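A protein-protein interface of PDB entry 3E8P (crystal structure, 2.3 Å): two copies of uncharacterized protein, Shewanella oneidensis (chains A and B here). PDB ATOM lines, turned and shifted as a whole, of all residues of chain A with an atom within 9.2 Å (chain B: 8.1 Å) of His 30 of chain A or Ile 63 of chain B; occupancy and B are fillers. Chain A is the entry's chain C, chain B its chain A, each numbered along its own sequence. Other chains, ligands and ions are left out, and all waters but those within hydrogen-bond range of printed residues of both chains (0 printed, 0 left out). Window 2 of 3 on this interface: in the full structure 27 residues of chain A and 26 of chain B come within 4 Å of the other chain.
The backbone carbonyl oxygen (O) of Ile 60 of chain B sits at hydrogen-bond distance from the backbone NH (N) of Phe 33 of chain A, 3.2 Å away.
Printed residues of chain A that touch a printed residue of chain B: His 30, Val 31, Pro 32 and Phe 33. Hydrophobic or aromatic side chains of chain A within 4 Å of the printed part of chain B: Val 31, Pro 32 and Phe 33. Printed residues of chain B that touch a printed residue of chain A: Pro 57, Ile 60, Gly 61 and Ile 63. Hydrophobic or aromatic side chains of chain B within 4 Å of the printed part of chain A: Ile 63. Among the printed residues, no Asp or Glu carboxylate lies within 4 Å of a Lys or Arg side-chain nitrogen of the other chain.
O of His 30 of chain A touches CD1 of Ile 63 of chain B, at 3.2 Å. Val 31 of chain A touches Ile 60 of chain B (CG1 to O, 3.9 Å). Gly 61 of chain B touches Val 31 of chain A (O to CG1, 3.5 Å). CB of Pro 32 of chain A touches O of Pro 57 of chain B, at 3.3 Å. O of Ile 60 of chain B touches CD of Pro 32 of chain A (3.3 Å).
N of Gly 61 of chain B lies within hydrogen-bond range of O of Ile 67 of chain B (2.9 Å). O of Ile 63 of chain B sits at hydrogen-bond distance from NE2 of Gln 66 of chain B, at 3.0 Å. O of Glu 25 of chain A lies within hydrogen-bond range of ND1 of His 30 of chain A, 3.2 Å away.
His 30 of chain A touches just one residue of chain B: Ile 63 (3.2 Å). Ile 63 of chain B touches one residue of chain A. Printed residues of chain B within 4 Å of Pro 32 of chain A: Pro 57 (3.3 Å) and Ile 60 (3.3 Å). Printed residues of chain B within 4 Å of Val 31 of chain A: Ile 60 and Gly 61. Printed residues of chain B within 4 Å of Phe 33 of chain A: Ile 60 (3.2 Å). The nearest printed residue of chain A that does not touch Gly 61 of chain B is Pro 32 of chain A (4.4 Å).
No position is printed for both chains. Of the 6 pairs that touch across the chains among the printed residues, none has its exchanged pair printed and touching as well.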
ATOM      1  N   LYS A  21       0.804 -33.283   4.065  1.00  0.00           N
ATOM      2  CA  LYS A  21       2.251 -33.354   3.885  1.00  0.00           C
ATOM      3  C   LYS A  21       2.722 -32.063   3.223  1.00  0.00           C
ATOM      4  O   LYS A  21       3.631 -31.394   3.708  1.00  0.00           O
ATOM      5  CB  LYS A  21       2.603 -34.557   3.001  1.00  0.00           C
ATOM      6  CG  LYS A  21       4.091 -34.768   2.747  1.00  0.00           C
ATOM      7  CD  LYS A  21       4.330 -35.968   1.823  1.00  0.00           C
ATOM      8  CE  LYS A  21       3.732 -35.737   0.438  1.00  0.00           C
ATOM      9  NZ  LYS A  21       3.859 -36.934  -0.444  1.00  0.00           N
ATOM     10  N   ARG A  22       2.082 -31.725   2.111  1.00  0.00           N
ATOM     11  CA  ARG A  22       2.404 -30.524   1.357  1.00  0.00           C
ATOM     12  C   ARG A  22       2.325 -29.283   2.244  1.00  0.00           C
ATOM     13  O   ARG A  22       3.320 -28.578   2.428  1.00  0.00           O
ATOM     14  CB  ARG A  22       1.441 -30.393   0.171  1.00  0.00           C
ATOM     15  CG  ARG A  22       1.498 -29.064  -0.562  1.00  0.00           C
ATOM     16  CD  ARG A  22       2.877 -28.785  -1.132  1.00  0.00           C
ATOM     17  NE  ARG A  22       2.944 -27.449  -1.720  1.00  0.00           N
ATOM     18  CZ  ARG A  22       4.065 -26.871  -2.141  1.00  0.00           C
ATOM     19  NH1 ARG A  22       5.223 -27.511  -2.046  1.00  0.00           N
ATOM     20  NH2 ARG A  22       4.030 -25.646  -2.649  1.00  0.00           N
ATOM     21  N   VAL A  23       1.143 -29.025   2.798  1.00  0.00           N
ATOM     22  CA  VAL A  23       0.933 -27.859   3.656  1.00  0.00           C
ATOM     23  C   VAL A  23       2.011 -27.701   4.730  1.00  0.00           C
ATOM     24  O   VAL A  23       2.414 -26.581   5.049  1.00  0.00           O
ATOM     25  CB  VAL A  23      -0.449 -27.922   4.351  1.00  0.00           C
ATOM     26  CG1 VAL A  23      -0.668 -26.677   5.186  1.00  0.00           C
ATOM     27  CG2 VAL A  23      -1.551 -28.054   3.313  1.00  0.00           C
ATOM     28  N   ALA A  24       2.482 -28.822   5.268  1.00  0.00           N
ATOM     29  CA  ALA A  24       3.500 -28.822   6.317  1.00  0.00           C
ATOM     30  C   ALA A  24       4.836 -28.201   5.908  1.00  0.00           C
ATOM     31  O   ALA A  24       5.347 -27.317   6.600  1.00  0.00           O
ATOM     32  CB  ALA A  24       3.720 -30.245   6.827  1.00  0.00           C
ATOM     33  N   GLU A  25       5.415 -28.661   4.801  1.00  0.00           N
ATOM     34  CA  GLU A  25       6.694 -28.110   4.362  1.00  0.00           C
ATOM     35  C   GLU A  25       6.528 -26.628   4.040  1.00  0.00           C
ATOM     36  O   GLU A  25       7.477 -25.849   4.145  1.00  0.00           O
ATOM     37  CB  GLU A  25       7.232 -28.864   3.136  1.00  0.00           C
ATOM     38  CG  GLU A  25       6.434 -28.683   1.850  1.00  0.00           C
ATOM     39  CD  GLU A  25       7.072 -29.396   0.666  1.00  0.00           C
ATOM     40  OE1 GLU A  25       6.503 -29.343  -0.445  1.00  0.00           O
ATOM     41  OE2 GLU A  25       8.146 -30.013   0.846  1.00  0.00           O
ATOM     42  N   VAL A  26       5.311 -26.249   3.653  1.00  0.00           N
ATOM     43  CA  VAL A  26       4.995 -24.860   3.329  1.00  0.00           C
ATOM     44  C   VAL A  26       5.260 -23.963   4.530  1.00  0.00           C
ATOM     45  O   VAL A  26       6.062 -23.036   4.456  1.00  0.00           O
ATOM     46  CB  VAL A  26       3.517 -24.701   2.923  1.00  0.00           C
ATOM     47  CG1 VAL A  26       3.208 -23.239   2.645  1.00  0.00           C
ATOM     48  CG2 VAL A  26       3.222 -25.550   1.703  1.00  0.00           C
ATOM     49  N   PHE A  27       4.575 -24.240   5.633  1.00  0.00           N
ATOM     50  CA  PHE A  27       4.746 -23.459   6.849  1.00  0.00           C
ATOM     51  C   PHE A  27       6.142 -23.667   7.411  1.00  0.00           C
ATOM     52  O   PHE A  27       6.773 -22.729   7.894  1.00  0.00           O
ATOM     53  CB  PHE A  27       3.702 -23.865   7.894  1.00  0.00           C
ATOM     54  CG  PHE A  27       2.314 -23.397   7.573  1.00  0.00           C
ATOM     55  CD1 PHE A  27       1.675 -23.807   6.405  1.00  0.00           C
ATOM     56  CD2 PHE A  27       1.650 -22.526   8.429  1.00  0.00           C
ATOM     57  CE1 PHE A  27       0.392 -23.353   6.094  1.00  0.00           C
ATOM     58  CE2 PHE A  27       0.369 -22.064   8.131  1.00  0.00           C
ATOM     59  CZ  PHE A  27      -0.262 -22.479   6.959  1.00  0.00           C
ATOM     60  N   ASP A  28       6.623 -24.903   7.330  1.00  0.00           N
ATOM     61  CA  ASP A  28       7.938 -25.254   7.848  1.00  0.00           C
ATOM     62  C   ASP A  28       9.123 -24.588   7.142  1.00  0.00           C
ATOM     63  O   ASP A  28      10.172 -24.389   7.759  1.00  0.00           O
ATOM     64  CB  ASP A  28       8.127 -26.773   7.800  1.00  0.00           C
ATOM     65  CG  ASP A  28       9.410 -27.222   8.478  1.00  0.00           C
ATOM     66  OD1 ASP A  28       9.521 -27.068   9.714  1.00  0.00           O
ATOM     67  OD2 ASP A  28      10.312 -27.725   7.774  1.00  0.00           O
ATOM     68  N   GLN A  29       8.970 -24.235   5.867  1.00  0.00           N
ATOM     69  CA  GLN A  29      10.086 -23.629   5.138  1.00  0.00           C
ATOM     70  C   GLN A  29       9.748 -22.496   4.161  1.00  0.00           C
ATOM     71  O   GLN A  29      10.582 -21.625   3.916  1.00  0.00           O
ATOM     72  CB  GLN A  29      10.860 -24.725   4.387  1.00  0.00           C
ATOM     73  CG  GLN A  29      11.390 -25.857   5.272  1.00  0.00           C
ATOM     74  CD  GLN A  29      12.717 -25.529   5.944  1.00  0.00           C
ATOM     75  OE1 GLN A  29      13.769 -25.532   5.300  1.00  0.00           O
ATOM     76  NE2 GLN A  29      12.672 -25.242   7.245  1.00  0.00           N
ATOM     77  N   HIS A  30       8.541 -22.501   3.605  1.00  0.00           N
ATOM     78  CA  HIS A  30       8.138 -21.466   2.648  1.00  0.00           C
ATOM     79  C   HIS A  30       7.676 -20.137   3.261  1.00  0.00           C
ATOM     80  O   HIS A  30       7.151 -19.280   2.548  1.00  0.00           O
ATOM     81  CB  HIS A  30       7.020 -21.995   1.751  1.00  0.00           C
ATOM     82  CG  HIS A  30       7.413 -23.174   0.917  1.00  0.00           C
ATOM     83  ND1 HIS A  30       8.103 -24.253   1.429  1.00  0.00           N
ATOM     84  CD2 HIS A  30       7.162 -23.468  -0.380  1.00  0.00           C
ATOM     85  CE1 HIS A  30       8.258 -25.160   0.482  1.00  0.00           C
ATOM     86  NE2 HIS A  30       7.696 -24.710  -0.625  1.00  0.00           N
ATOM     87  N   VAL A  31       7.862 -19.958   4.566  1.00  0.00           N
ATOM     88  CA  VAL A  31       7.443 -18.722   5.229  1.00  0.00           C
ATOM     89  C   VAL A  31       8.636 -17.971   5.818  1.00  0.00           C
ATOM     90  O   VAL A  31       9.217 -18.388   6.823  1.00  0.00           O
ATOM     91  CB  VAL A  31       6.429 -19.004   6.363  1.00  0.00           C
ATOM     92  CG1 VAL A  31       6.010 -17.698   7.028  1.00  0.00           C
ATOM     93  CG2 VAL A  31       5.211 -19.734   5.804  1.00  0.00           C
ATOM     94  N   PRO A  32       9.004 -16.834   5.210  1.00  0.00           N
ATOM     95  CA  PRO A  32      10.134 -16.032   5.679  1.00  0.00           C
ATOM     96  C   PRO A  32      10.166 -15.747   7.178  1.00  0.00           C
ATOM     97  O   PRO A  32      11.192 -15.941   7.825  1.00  0.00           O
ATOM     98  CB  PRO A  32      10.015 -14.755   4.848  1.00  0.00           C
ATOM     99  CG  PRO A  32       9.446 -15.246   3.563  1.00  0.00           C
ATOM    100  CD  PRO A  32       8.382 -16.221   4.025  1.00  0.00           C
ATOM    101  N   PHE A  33       9.052 -15.288   7.742  1.00  0.00           N
ATOM    102  CA  PHE A  33       9.043 -14.969   9.166  1.00  0.00           C
ATOM    103  C   PHE A  33       9.318 -16.188  10.040  1.00  0.00           C
ATOM    104  O   PHE A  33       9.883 -16.057  11.126  1.00  0.00           O
ATOM    105  CB  PHE A  33       7.717 -14.322   9.566  1.00  0.00           C
ATOM    106  CG  PHE A  33       7.730 -13.715  10.949  1.00  0.00           C
ATOM    107  CD1 PHE A  33       8.661 -12.736  11.286  1.00  0.00           C
ATOM    108  CD2 PHE A  33       6.788 -14.098  11.902  1.00  0.00           C
ATOM    109  CE1 PHE A  33       8.657 -12.142  12.559  1.00  0.00           C
ATOM    110  CE2 PHE A  33       6.769 -13.513  13.174  1.00  0.00           C
ATOM    111  CZ  PHE A  33       7.705 -12.533  13.503  1.00  0.00           C
ATOM    112  N   HIS A  34       8.921 -17.367   9.572  1.00  0.00           N
ATOM    113  CA  HIS A  34       9.161 -18.591  10.334  1.00  0.00           C
ATOM    114  C   HIS A  34      10.653 -18.897  10.386  1.00  0.00           C
ATOM    115  O   HIS A  34      11.162 -19.368  11.408  1.00  0.00           O
ATOM    116  CB  HIS A  34       8.408 -19.783   9.723  1.00  0.00           C
ATOM    117  CG  HIS A  34       6.919 -19.690   9.857  1.00  0.00           C
ATOM    118  ND1 HIS A  34       6.065 -20.676   9.412  1.00  0.00           N
ATOM    119  CD2 HIS A  34       6.131 -18.709  10.359  1.00  0.00           C
ATOM    120  CE1 HIS A  34       4.817 -20.306   9.630  1.00  0.00           C
ATOM    121  NE2 HIS A  34       4.829 -19.116  10.205  1.00  0.00           N
ATOM    122  N   ASN A  35      11.353 -18.631   9.285  1.00  0.00           N
ATOM    123  CA  ASN A  35      12.795 -18.860   9.231  1.00  0.00           C
ATOM    124  C   ASN A  35      13.547 -17.855  10.098  1.00  0.00           C
ATOM    125  O   ASN A  35      14.570 -18.182  10.692  1.00  0.00           O
ATOM    126  CB  ASN A  35      13.310 -18.770   7.797  1.00  0.00           C
ATOM    127  CG  ASN A  35      14.827 -18.726   7.733  1.00  0.00           C
ATOM    128  OD1 ASN A  35      15.438 -17.672   7.923  1.00  0.00           O
ATOM    129  ND2 ASN A  35      15.444 -19.875   7.484  1.00  0.00           N
ATOM    130  N   LEU A  39      10.899 -21.049  13.722  1.00  0.00           N
ATOM    131  CA  LEU A  39       9.669 -21.790  13.950  1.00  0.00           C
ATOM    132  C   LEU A  39       9.653 -23.041  13.078  1.00  0.00           C
ATOM    133  O   LEU A  39       9.819 -22.964  11.866  1.00  0.00           O
ATOM    134  CB  LEU A  39       8.463 -20.893  13.638  1.00  0.00           C
ATOM    135  CG  LEU A  39       7.050 -21.403  13.942  1.00  0.00           C
ATOM    136  CD1 LEU A  39       6.088 -20.231  14.041  1.00  0.00           C
ATOM    137  CD2 LEU A  39       6.603 -22.364  12.859  1.00  0.00           C
ATOM    138  N   ILE A  41       7.707 -26.940  12.134  1.00  0.00           N
ATOM    139  CA  ILE A  41       6.523 -27.783  12.197  1.00  0.00           C
ATOM    140  C   ILE A  41       7.029 -29.190  12.530  1.00  0.00           C
ATOM    141  O   ILE A  41       7.327 -29.974  11.635  1.00  0.00           O
ATOM    142  CB  ILE A  41       5.797 -27.811  10.842  1.00  0.00           C
ATOM    143  CG1 ILE A  41       5.539 -26.382  10.357  1.00  0.00           C
ATOM    144  CG2 ILE A  41       4.491 -28.575  10.967  1.00  0.00           C
ATOM    145  CD1 ILE A  41       4.714 -25.532  11.314  1.00  0.00           C
ATOM    146  N   PRO B  57      11.949  -8.298   3.754  1.00  0.00           N
ATOM    147  CA  PRO B  57      11.704  -9.690   3.365  1.00  0.00           C
ATOM    148  C   PRO B  57      11.491 -10.680   4.515  1.00  0.00           C
ATOM    149  O   PRO B  57      10.602 -11.526   4.445  1.00  0.00           O
ATOM    150  CB  PRO B  57      12.937 -10.030   2.519  1.00  0.00           C
ATOM    151  CG  PRO B  57      13.286  -8.708   1.902  1.00  0.00           C
ATOM    152  CD  PRO B  57      13.143  -7.766   3.073  1.00  0.00           C
ATOM    153  N   ILE B  60       7.773 -11.265   5.999  1.00  0.00           N
ATOM    154  CA  ILE B  60       6.668 -11.736   5.164  1.00  0.00           C
ATOM    155  C   ILE B  60       6.054 -13.070   5.585  1.00  0.00           C
ATOM    156  O   ILE B  60       6.761 -14.015   5.933  1.00  0.00           O
ATOM    157  CB  ILE B  60       7.118 -11.844   3.696  1.00  0.00           C
ATOM    158  CG1 ILE B  60       7.485 -10.457   3.173  1.00  0.00           C
ATOM    159  CG2 ILE B  60       6.014 -12.461   2.843  1.00  0.00           C
ATOM    160  CD1 ILE B  60       7.982 -10.466   1.749  1.00  0.00           C
ATOM    161  N   GLY B  61       4.726 -13.138   5.536  1.00  0.00           N
ATOM    162  CA  GLY B  61       4.028 -14.361   5.889  1.00  0.00           C
ATOM    163  C   GLY B  61       3.683 -15.152   4.642  1.00  0.00           C
ATOM    164  O   GLY B  61       4.022 -16.326   4.522  1.00  0.00           O
ATOM    165  N   ASN B  62       3.004 -14.503   3.705  1.00  0.00           N
ATOM    166  CA  ASN B  62       2.626 -15.151   2.458  1.00  0.00           C
ATOM    167  C   ASN B  62       3.435 -14.534   1.318  1.00  0.00           C
ATOM    168  O   ASN B  62       3.297 -13.348   1.014  1.00  0.00           O
ATOM    169  CB  ASN B  62       1.130 -14.971   2.213  1.00  0.00           C
ATOM    170  CG  ASN B  62       0.664 -15.630   0.936  1.00  0.00           C
ATOM    171  OD1 ASN B  62       1.022 -15.207  -0.162  1.00  0.00           O
ATOM    172  ND2 ASN B  62      -0.140 -16.679   1.073  1.00  0.00           N
ATOM    173  N   ILE B  63       4.291 -15.349   0.705  1.00  0.00           N
ATOM    174  CA  ILE B  63       5.150 -14.910  -0.392  1.00  0.00           C
ATOM    175  C   ILE B  63       4.386 -14.331  -1.579  1.00  0.00           C
ATOM    176  O   ILE B  63       4.747 -13.276  -2.095  1.00  0.00           O
ATOM    177  CB  ILE B  63       6.046 -16.079  -0.884  1.00  0.00           C
ATOM    178  CG1 ILE B  63       7.079 -16.419   0.190  1.00  0.00           C
ATOM    179  CG2 ILE B  63       6.745 -15.712  -2.177  1.00  0.00           C
ATOM    180  CD1 ILE B  63       7.906 -17.660  -0.118  1.00  0.00           C
ATOM    181  N   HIS B  64       3.332 -15.015  -2.007  1.00  0.00           N
ATOM    182  CA  HIS B  64       2.544 -14.553  -3.146  1.00  0.00           C
ATOM    183  C   HIS B  64       1.872 -13.202  -2.909  1.00  0.00           C
ATOM    184  O   HIS B  64       2.018 -12.280  -3.708  1.00  0.00           O
ATOM    185  CB  HIS B  64       1.488 -15.603  -3.514  1.00  0.00           C
ATOM    186  CG  HIS B  64       0.666 -15.244  -4.715  1.00  0.00           C
ATOM    187  ND1 HIS B  64      -0.204 -14.175  -4.732  1.00  0.00           N
ATOM    188  CD2 HIS B  64       0.578 -15.820  -5.938  1.00  0.00           C
ATOM    189  CE1 HIS B  64      -0.794 -14.109  -5.912  1.00  0.00           C
ATOM    190  NE2 HIS B  64      -0.338 -15.095  -6.663  1.00  0.00           N
ATOM    191  N   GLN B  65       1.144 -13.083  -1.803  1.00  0.00           N
ATOM    192  CA  GLN B  65       0.431 -11.846  -1.476  1.00  0.00           C
ATOM    193  C   GLN B  65       1.336 -10.749  -0.912  1.00  0.00           C
ATOM    194  O   GLN B  65       0.916  -9.603  -0.795  1.00  0.00           O
ATOM    195  CB  GLN B  65      -0.682 -12.134  -0.459  1.00  0.00           C
ATOM    196  CG  GLN B  65      -1.685 -13.207  -0.869  1.00  0.00           C
ATOM    197  CD  GLN B  65      -2.624 -12.756  -1.975  1.00  0.00           C
ATOM    198  OE1 GLN B  65      -3.469 -13.525  -2.441  1.00  0.00           O
ATOM    199  NE2 GLN B  65      -2.483 -11.502  -2.400  1.00  0.00           N
ATOM    200  N   GLN B  66       2.567 -11.100  -0.559  1.00  0.00           N
ATOM    201  CA  GLN B  66       3.501 -10.139   0.015  1.00  0.00           C
ATOM    202  C   GLN B  66       2.872  -9.436   1.216  1.00  0.00           C
ATOM    203  O   GLN B  66       2.928  -8.212   1.338  1.00  0.00           O
ATOM    204  CB  GLN B  66       3.932  -9.098  -1.030  1.00  0.00           C
ATOM    205  CG  GLN B  66       4.976  -9.607  -2.022  1.00  0.00           C
ATOM    206  CD  GLN B  66       6.321  -9.891  -1.368  1.00  0.00           C
ATOM    207  OE1 GLN B  66       7.036  -8.977  -0.965  1.00  0.00           O
ATOM    208  NE2 GLN B  66       6.664 -11.166  -1.254  1.00  0.00           N
ATOM    209  N   ILE B  67       2.262 -10.214   2.101  1.00  0.00           N
ATOM    210  CA  ILE B  67       1.649  -9.630   3.283  1.00  0.00           C
ATOM    211  C   ILE B  67       2.495  -9.893   4.524  1.00  0.00           C
ATOM    212  O   ILE B  67       3.243 -10.870   4.607  1.00  0.00           O
ATOM    213  CB  ILE B  67       0.223 -10.170   3.520  1.00  0.00           C
ATOM    214  CG1 ILE B  67       0.252 -11.676   3.704  1.00  0.00           C
ATOM    215  CG2 ILE B  67      -0.658  -9.854   2.335  1.00  0.00           C
ATOM    216  CD1 ILE B  67      -1.078 -12.237   4.094  1.00  0.00           C
